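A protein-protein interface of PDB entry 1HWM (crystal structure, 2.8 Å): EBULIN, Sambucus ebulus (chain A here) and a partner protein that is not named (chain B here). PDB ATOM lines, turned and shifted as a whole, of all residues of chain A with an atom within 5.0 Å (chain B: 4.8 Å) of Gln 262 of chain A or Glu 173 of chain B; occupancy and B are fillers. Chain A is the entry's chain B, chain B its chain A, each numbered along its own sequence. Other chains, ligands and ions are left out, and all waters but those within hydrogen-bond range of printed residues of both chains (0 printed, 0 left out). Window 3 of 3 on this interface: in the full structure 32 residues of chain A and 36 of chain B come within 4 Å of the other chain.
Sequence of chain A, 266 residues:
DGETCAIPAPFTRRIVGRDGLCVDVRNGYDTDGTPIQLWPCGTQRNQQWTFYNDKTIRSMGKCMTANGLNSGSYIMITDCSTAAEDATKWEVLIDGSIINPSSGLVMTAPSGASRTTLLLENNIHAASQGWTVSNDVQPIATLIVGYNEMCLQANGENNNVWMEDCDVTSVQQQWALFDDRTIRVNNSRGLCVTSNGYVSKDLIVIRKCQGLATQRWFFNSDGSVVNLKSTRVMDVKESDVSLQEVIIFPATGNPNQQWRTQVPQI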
ATOM      1  N   THR A 142      11.459   6.185   8.868  1.00  0.00           N
ATOM      2  CA  THR A 142      11.431   6.404  10.309  1.00  0.00           C
ATOM      3  C   THR A 142      10.560   7.545  10.809  1.00  0.00           C
ATOM      4  O   THR A 142       9.999   8.326  10.039  1.00  0.00           O
ATOM      5  CB  THR A 142      12.841   6.666  10.876  1.00  0.00           C
ATOM      6  OG1 THR A 142      13.325   7.919  10.379  1.00  0.00           O
ATOM      7  CG2 THR A 142      13.795   5.555  10.497  1.00  0.00           C
ATOM      8  N   LEU A 143      10.468   7.611  12.132  1.00  0.00           N
ATOM      9  CA  LEU A 143       9.722   8.639  12.839  1.00  0.00           C
ATOM     10  C   LEU A 143      10.795   9.563  13.395  1.00  0.00           C
ATOM     11  O   LEU A 143      11.730   9.099  14.047  1.00  0.00           O
ATOM     12  CB  LEU A 143       8.945   8.021  14.004  1.00  0.00           C
ATOM     13  CG  LEU A 143       7.415   8.000  13.983  1.00  0.00           C
ATOM     14  CD1 LEU A 143       6.917   7.786  15.403  1.00  0.00           C
ATOM     15  CD2 LEU A 143       6.866   9.299  13.415  1.00  0.00           C
ATOM     16  N   VAL A 145      11.509  11.823  16.055  1.00  0.00           N
ATOM     17  CA  VAL A 145      11.094  12.316  17.363  1.00  0.00           C
ATOM     18  C   VAL A 145      12.055  13.371  17.904  1.00  0.00           C
ATOM     19  O   VAL A 145      13.264  13.293  17.684  1.00  0.00           O
ATOM     20  CB  VAL A 145      11.007  11.161  18.385  1.00  0.00           C
ATOM     21  CG1 VAL A 145      10.324  11.639  19.656  1.00  0.00           C
ATOM     22  CG2 VAL A 145      10.250   9.987  17.778  1.00  0.00           C
ATOM     23  N   ARG A 260      15.799  11.813  17.819  1.00  0.00           N
ATOM     24  CA  ARG A 260      15.927  10.363  17.832  1.00  0.00           C
ATOM     25  C   ARG A 260      15.141   9.749  16.682  1.00  0.00           C
ATOM     26  O   ARG A 260      13.923   9.897  16.603  1.00  0.00           O
ATOM     27  CB  ARG A 260      15.419   9.806  19.164  1.00  0.00           C
ATOM     28  CG  ARG A 260      15.175   8.306  19.160  1.00  0.00           C
ATOM     29  CD  ARG A 260      16.471   7.538  19.345  1.00  0.00           C
ATOM     30  NE  ARG A 260      16.648   6.514  18.320  1.00  0.00           N
ATOM     31  CZ  ARG A 260      17.695   6.443  17.505  1.00  0.00           C
ATOM     32  NH1 ARG A 260      18.668   7.340  17.595  1.00  0.00           N
ATOM     33  NH2 ARG A 260      17.767   5.478  16.596  1.00  0.00           N
ATOM     34  N   THR A 261      15.845   9.061  15.790  1.00  0.00           N
ATOM     35  CA  THR A 261      15.207   8.428  14.644  1.00  0.00           C
ATOM     36  C   THR A 261      14.634   7.062  15.013  1.00  0.00           C
ATOM     37  O   THR A 261      15.354   6.064  15.038  1.00  0.00           O
ATOM     38  CB  THR A 261      16.209   8.254  13.484  1.00  0.00           C
ATOM     39  OG1 THR A 261      17.484   7.858  14.003  1.00  0.00           O
ATOM     40  CG2 THR A 261      16.366   9.558  12.720  1.00  0.00           C
ATOM     41  N   GLN A 262      13.336   7.021  15.303  1.00  0.00           N
ATOM     42  CA  GLN A 262      12.677   5.770  15.667  1.00  0.00           C
ATOM     43  C   GLN A 262      12.144   5.062  14.428  1.00  0.00           C
ATOM     44  O   GLN A 262      11.070   5.390  13.925  1.00  0.00           O
ATOM     45  CB  GLN A 262      11.524   6.038  16.637  1.00  0.00           C
ATOM     46  CG  GLN A 262      11.951   6.204  18.085  1.00  0.00           C
ATOM     47  CD  GLN A 262      12.903   5.121  18.544  1.00  0.00           C
ATOM     48  OE1 GLN A 262      12.490   4.109  19.106  1.00  0.00           O
ATOM     49  NE2 GLN A 262      14.190   5.330  18.305  1.00  0.00           N
ATOM     50  N   VAL A 263      12.899   4.085  13.945  1.00  0.00           N
ATOM     51  CA  VAL A 263      12.507   3.341  12.758  1.00  0.00           C
ATOM     52  C   VAL A 263      11.210   2.568  12.990  1.00  0.00           C
ATOM     53  O   VAL A 263      11.118   1.762  13.909  1.00  0.00           O
ATOM     54  CB  VAL A 263      13.624   2.355  12.334  1.00  0.00           C
ATOM     55  CG1 VAL A 263      14.926   3.110  12.130  1.00  0.00           C
ATOM     56  CG2 VAL A 263      13.815   1.281  13.394  1.00  0.00           C
ATOM     57  N   PRO A 264      10.175   2.835  12.176  1.00  0.00           N
ATOM     58  CA  PRO A 264       8.904   2.127  12.333  1.00  0.00           C
ATOM     59  C   PRO A 264       8.929   0.814  11.554  1.00  0.00           C
ATOM     60  O   PRO A 264       8.288  -0.163  11.942  1.00  0.00           O
ATOM     61  CB  PRO A 264       7.885   3.109  11.769  1.00  0.00           C
ATOM     62  CG  PRO A 264       8.640   3.835  10.703  1.00  0.00           C
ATOM     63  CD  PRO A 264      10.109   3.827  11.093  1.00  0.00           C
ATOM     64  N   TYR B 169      17.772   4.155  21.344  1.00  0.00           N
ATOM     65  CA  TYR B 169      16.522   3.644  20.794  1.00  0.00           C
ATOM     66  C   TYR B 169      15.723   3.107  21.973  1.00  0.00           C
ATOM     67  O   TYR B 169      14.522   3.347  22.091  1.00  0.00           O
ATOM     68  CB  TYR B 169      16.796   2.518  19.795  1.00  0.00           C
ATOM     69  CG  TYR B 169      15.572   1.731  19.382  1.00  0.00           C
ATOM     70  CD1 TYR B 169      14.901   2.021  18.194  1.00  0.00           C
ATOM     71  CD2 TYR B 169      15.097   0.677  20.164  1.00  0.00           C
ATOM     72  CE1 TYR B 169      13.792   1.281  17.793  1.00  0.00           C
ATOM     73  CE2 TYR B 169      13.989  -0.069  19.773  1.00  0.00           C
ATOM     74  CZ  TYR B 169      13.342   0.237  18.587  1.00  0.00           C
ATOM     75  OH  TYR B 169      12.249  -0.501  18.194  1.00  0.00           O
ATOM     76  N   ILE B 170      16.410   2.371  22.841  1.00  0.00           N
ATOM     77  CA  ILE B 170      15.793   1.807  24.033  1.00  0.00           C
ATOM     78  C   ILE B 170      15.399   2.971  24.937  1.00  0.00           C
ATOM     79  O   ILE B 170      14.299   3.003  25.487  1.00  0.00           O
ATOM     80  CB  ILE B 170      16.777   0.890  24.796  1.00  0.00           C
ATOM     81  CG1 ILE B 170      17.351  -0.165  23.846  1.00  0.00           C
ATOM     82  CG2 ILE B 170      16.069   0.231  25.970  1.00  0.00           C
ATOM     83  CD1 ILE B 170      18.260  -1.173  24.521  1.00  0.00           C
ATOM     84  N   GLU B 171      16.309   3.929  25.085  1.00  0.00           N
ATOM     85  CA  GLU B 171      16.057   5.103  25.910  1.00  0.00           C
ATOM     86  C   GLU B 171      14.713   5.712  25.530  1.00  0.00           C
ATOM     87  O   GLU B 171      13.953   6.152  26.391  1.00  0.00           O
ATOM     88  CB  GLU B 171      17.165   6.136  25.706  1.00  0.00           C
ATOM     89  CG  GLU B 171      16.897   7.478  26.362  1.00  0.00           C
ATOM     90  CD  GLU B 171      18.164   8.279  26.573  1.00  0.00           C
ATOM     91  OE1 GLU B 171      19.183   7.961  25.927  1.00  0.00           O
ATOM     92  OE2 GLU B 171      18.140   9.227  27.385  1.00  0.00           O
ATOM     93  N   GLN B 172      14.433   5.735  24.231  1.00  0.00           N
ATOM     94  CA  GLN B 172      13.182   6.276  23.722  1.00  0.00           C
ATOM     95  C   GLN B 172      12.007   5.426  24.187  1.00  0.00           C
ATOM     96  O   GLN B 172      11.113   5.913  24.878  1.00  0.00           O
ATOM     97  CB  GLN B 172      13.207   6.318  22.193  1.00  0.00           C
ATOM     98  CG  GLN B 172      11.995   6.994  21.573  1.00  0.00           C
ATOM     99  CD  GLN B 172      11.621   8.279  22.281  1.00  0.00           C
ATOM    100  OE1 GLN B 172      12.485   9.041  22.714  1.00  0.00           O
ATOM    101  NE2 GLN B 172      10.325   8.529  22.400  1.00  0.00           N
ATOM    102  N   GLU B 173      12.014   4.153  23.805  1.00  0.00           N
ATOM    103  CA  GLU B 173      10.945   3.238  24.184  1.00  0.00           C
ATOM    104  C   GLU B 173      10.589   3.411  25.655  1.00  0.00           C
ATOM    105  O   GLU B 173       9.430   3.635  26.003  1.00  0.00           O
ATOM    106  CB  GLU B 173      11.371   1.793  23.926  1.00  0.00           C
ATOM    107  CG  GLU B 173      10.316   0.956  23.223  1.00  0.00           C
ATOM    108  CD  GLU B 173      10.580   0.823  21.738  1.00  0.00           C
ATOM    109  OE1 GLU B 173      10.498   1.847  21.023  1.00  0.00           O
ATOM    110  OE2 GLU B 173      10.870  -0.306  21.286  1.00  0.00           O
ATOM    111  N   VAL B 174      11.597   3.309  26.516  1.00  0.00           N
ATOM    112  CA  VAL B 174      11.399   3.458  27.951  1.00  0.00           C
ATOM    113  C   VAL B 174      10.851   4.840  28.276  1.00  0.00           C
ATOM    114  O   VAL B 174       9.905   4.978  29.051  1.00  0.00           O
ATOM    115  CB  VAL B 174      12.719   3.266  28.719  1.00  0.00           C
ATOM    116  CG1 VAL B 174      12.517   3.594  30.189  1.00  0.00           C
ATOM    117  CG2 VAL B 174      13.214   1.838  28.552  1.00  0.00           C
ATOM    118  N   ARG B 175      11.455   5.865  27.685  1.00  0.00           N
ATOM    119  CA  ARG B 175      11.024   7.239  27.908  1.00  0.00           C
ATOM    120  C   ARG B 175       9.524   7.370  27.663  1.00  0.00           C
ATOM    121  O   ARG B 175       8.795   7.934  28.481  1.00  0.00           O
ATOM    122  CB  ARG B 175      11.785   8.186  26.979  1.00  0.00           C
ATOM    123  CG  ARG B 175      12.276   9.457  27.653  1.00  0.00           C
ATOM    124  CD  ARG B 175      13.459  10.060  26.911  1.00  0.00           C
ATOM    125  NE  ARG B 175      13.070  11.205  26.090  1.00  0.00           N
ATOM    126  CZ  ARG B 175      12.720  12.392  26.576  1.00  0.00           C
ATOM    127  NH1 ARG B 175      12.708  12.596  27.887  1.00  0.00           N
ATOM    128  NH2 ARG B 175      12.379  13.378  25.751  1.00  0.00           N
ATOM    129  N   ARG B 176       9.068   6.837  26.534  1.00  0.00           N
ATOM    130  CA  ARG B 176       7.656   6.888  26.169  1.00  0.00           C
ATOM    131  C   ARG B 176       6.814   6.090  27.159  1.00  0.00           C
ATOM    132  O   ARG B 176       5.657   6.428  27.419  1.00  0.00           O
ATOM    133  CB  ARG B 176       7.465   6.334  24.754  1.00  0.00           C
ATOM    134  CG  ARG B 176       6.013   6.142  24.341  1.00  0.00           C
ATOM    135  CD  ARG B 176       5.447   7.398  23.689  1.00  0.00           C
ATOM    136  NE  ARG B 176       6.293   7.885  22.601  1.00  0.00           N
ATOM    137  CZ  ARG B 176       6.671   9.153  22.459  1.00  0.00           C
ATOM    138  NH1 ARG B 176       6.282  10.070  23.335  1.00  0.00           N
ATOM    139  NH2 ARG B 176       7.443   9.505  21.439  1.00  0.00           N
ATOM    140  N   SER B 177       7.398   5.030  27.706  1.00  0.00           N
ATOM    141  CA  SER B 177       6.702   4.183  28.668  1.00  0.00           C
ATOM    142  C   SER B 177       6.336   4.974  29.918  1.00  0.00           C
ATOM    143  O   SER B 177       5.296   4.735  30.532  1.00  0.00           O
ATOM    144  CB  SER B 177       7.575   2.979  29.047  1.00  0.00           C
ATOM    145  OG  SER B 177       8.453   3.292  30.113  1.00  0.00           O
ATOM    146  N   PHE B 184       5.440  -2.392  27.975  1.00  0.00           N
ATOM    147  CA  PHE B 184       5.787  -3.019  26.709  1.00  0.00           C
ATOM    148  C   PHE B 184       6.788  -4.156  26.856  1.00  0.00           C
ATOM    149  O   PHE B 184       7.590  -4.183  27.789  1.00  0.00           O
ATOM    150  CB  PHE B 184       6.368  -1.969  25.760  1.00  0.00           C
ATOM    151  CG  PHE B 184       7.741  -1.493  26.152  1.00  0.00           C
ATOM    152  CD1 PHE B 184       8.877  -2.077  25.606  1.00  0.00           C
ATOM    153  CD2 PHE B 184       7.897  -0.476  27.088  1.00  0.00           C
ATOM    154  CE1 PHE B 184      10.146  -1.654  25.986  1.00  0.00           C
ATOM    155  CE2 PHE B 184       9.164  -0.050  27.471  1.00  0.00           C
ATOM    156  CZ  PHE B 184      10.288  -0.640  26.921  1.00  0.00           C
ATOM    157  N   ASN B 187      10.758  -5.859  21.546  1.00  0.00           N
ATOM    158  CA  ASN B 187      10.497  -6.385  20.210  1.00  0.00           C
ATOM    159  C   ASN B 187      11.756  -7.021  19.622  1.00  0.00           C
ATOM    160  O   ASN B 187      12.850  -6.880  20.169  1.00  0.00           O
ATOM    161  CB  ASN B 187       9.987  -5.276  19.283  1.00  0.00           C
ATOM    162  CG  ASN B 187      10.926  -4.091  19.213  1.00  0.00           C
ATOM    163  OD1 ASN B 187      12.135  -4.255  19.078  1.00  0.00           O
ATOM    164  ND2 ASN B 187      10.371  -2.890  19.302  1.00  0.00           N
ATOM    165  N   MET B 190      14.844  -4.615  19.227  1.00  0.00           N
ATOM    166  CA  MET B 190      15.415  -4.231  20.513  1.00  0.00           C
ATOM    167  C   MET B 190      16.377  -5.301  21.012  1.00  0.00           C
ATOM    168  O   MET B 190      17.573  -5.051  21.169  1.00  0.00           O
ATOM    169  CB  MET B 190      14.296  -4.017  21.539  1.00  0.00           C
ATOM    170  CG  MET B 190      14.775  -3.888  22.975  1.00  0.00           C
ATOM    171  SD  MET B 190      13.649  -2.929  24.011  1.00  0.00           S
ATOM    172  CE  MET B 190      14.283  -3.315  25.643  1.00  0.00           C
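The side-chain hydroxyl (OH) of Tyr 169 of chain B sits at hydrogen-bond distance from the side-chain carboxylate (OE2) of Glu 173 of chain B (3.4 Å). OH of Tyr 169 of chain B lies within hydrogen-bond range of ND2 of Asn 187 of chain B (3.2 Å). NH2 of Arg 176 of chain B sits close to NE2 of Gln 172 of chain B, at 3.2 Å. The side-chain carboxylate of Glu 173 of chain B sits at hydrogen-bond distance from the side-chain amide nitrogen of Asn 187 of chain B (3.3 Å). N of Arg 260 of chain A is in hydrogen-bond range of O of Val 145 of chain A (2.9 Å). The guanidinium group (NE) of Arg 260 of chain A lies close to the side-chain amide nitrogen (NE2) of Gln 262 of chain A (2.7 Å).
Tyr 169 of chain B touches Arg 260 of chain A. Tyr 169 of chain B touches Gln 262 of chain A (CD1 to OE1, 3.3 Å). Gln 262 of chain A touches Gln 172 of chain B (CG to CG, 3.6 Å). OE1 of Glu 173 of chain B touches OE1 of Gln 262 of chain A, 3.6 Å away.
Of chain B, only Tyr 169 (3.3 Å), Gln 172 (3.6 Å) and Glu 173 (3.6 Å) come within 4 Å of Gln 262 of chain A. Of chain A, only Gln 262 (3.6 Å) comes within 4 Å of Glu 173 of chain B. Printed residues of chain B within 4 Å of Arg 260 of chain A: Tyr 169 (3.8 Å). Of the printed residues of chain A, Tyr 169 of chain B touches Arg 260 and Gln 262. Of the printed residues of chain A, Gln 172 of chain B touches Gln 262. The nearest printed residue of chain A that does not touch Glu 173 of chain B is Arg 260 of chain A (7.0 Å).
Of the 12 printed residues of chain B, 3 touch a printed residue of chain A. Hydrophobic or aromatic side chains of chain B within 4 Å of the printed part of chain A: Tyr 169. Among the printed residues, 4 pairs touch across the chains. Among the printed residues, no Asp or Glu carboxylate lies within 4 Å of a Lys or Arg side-chain nitrogen of the other chain.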
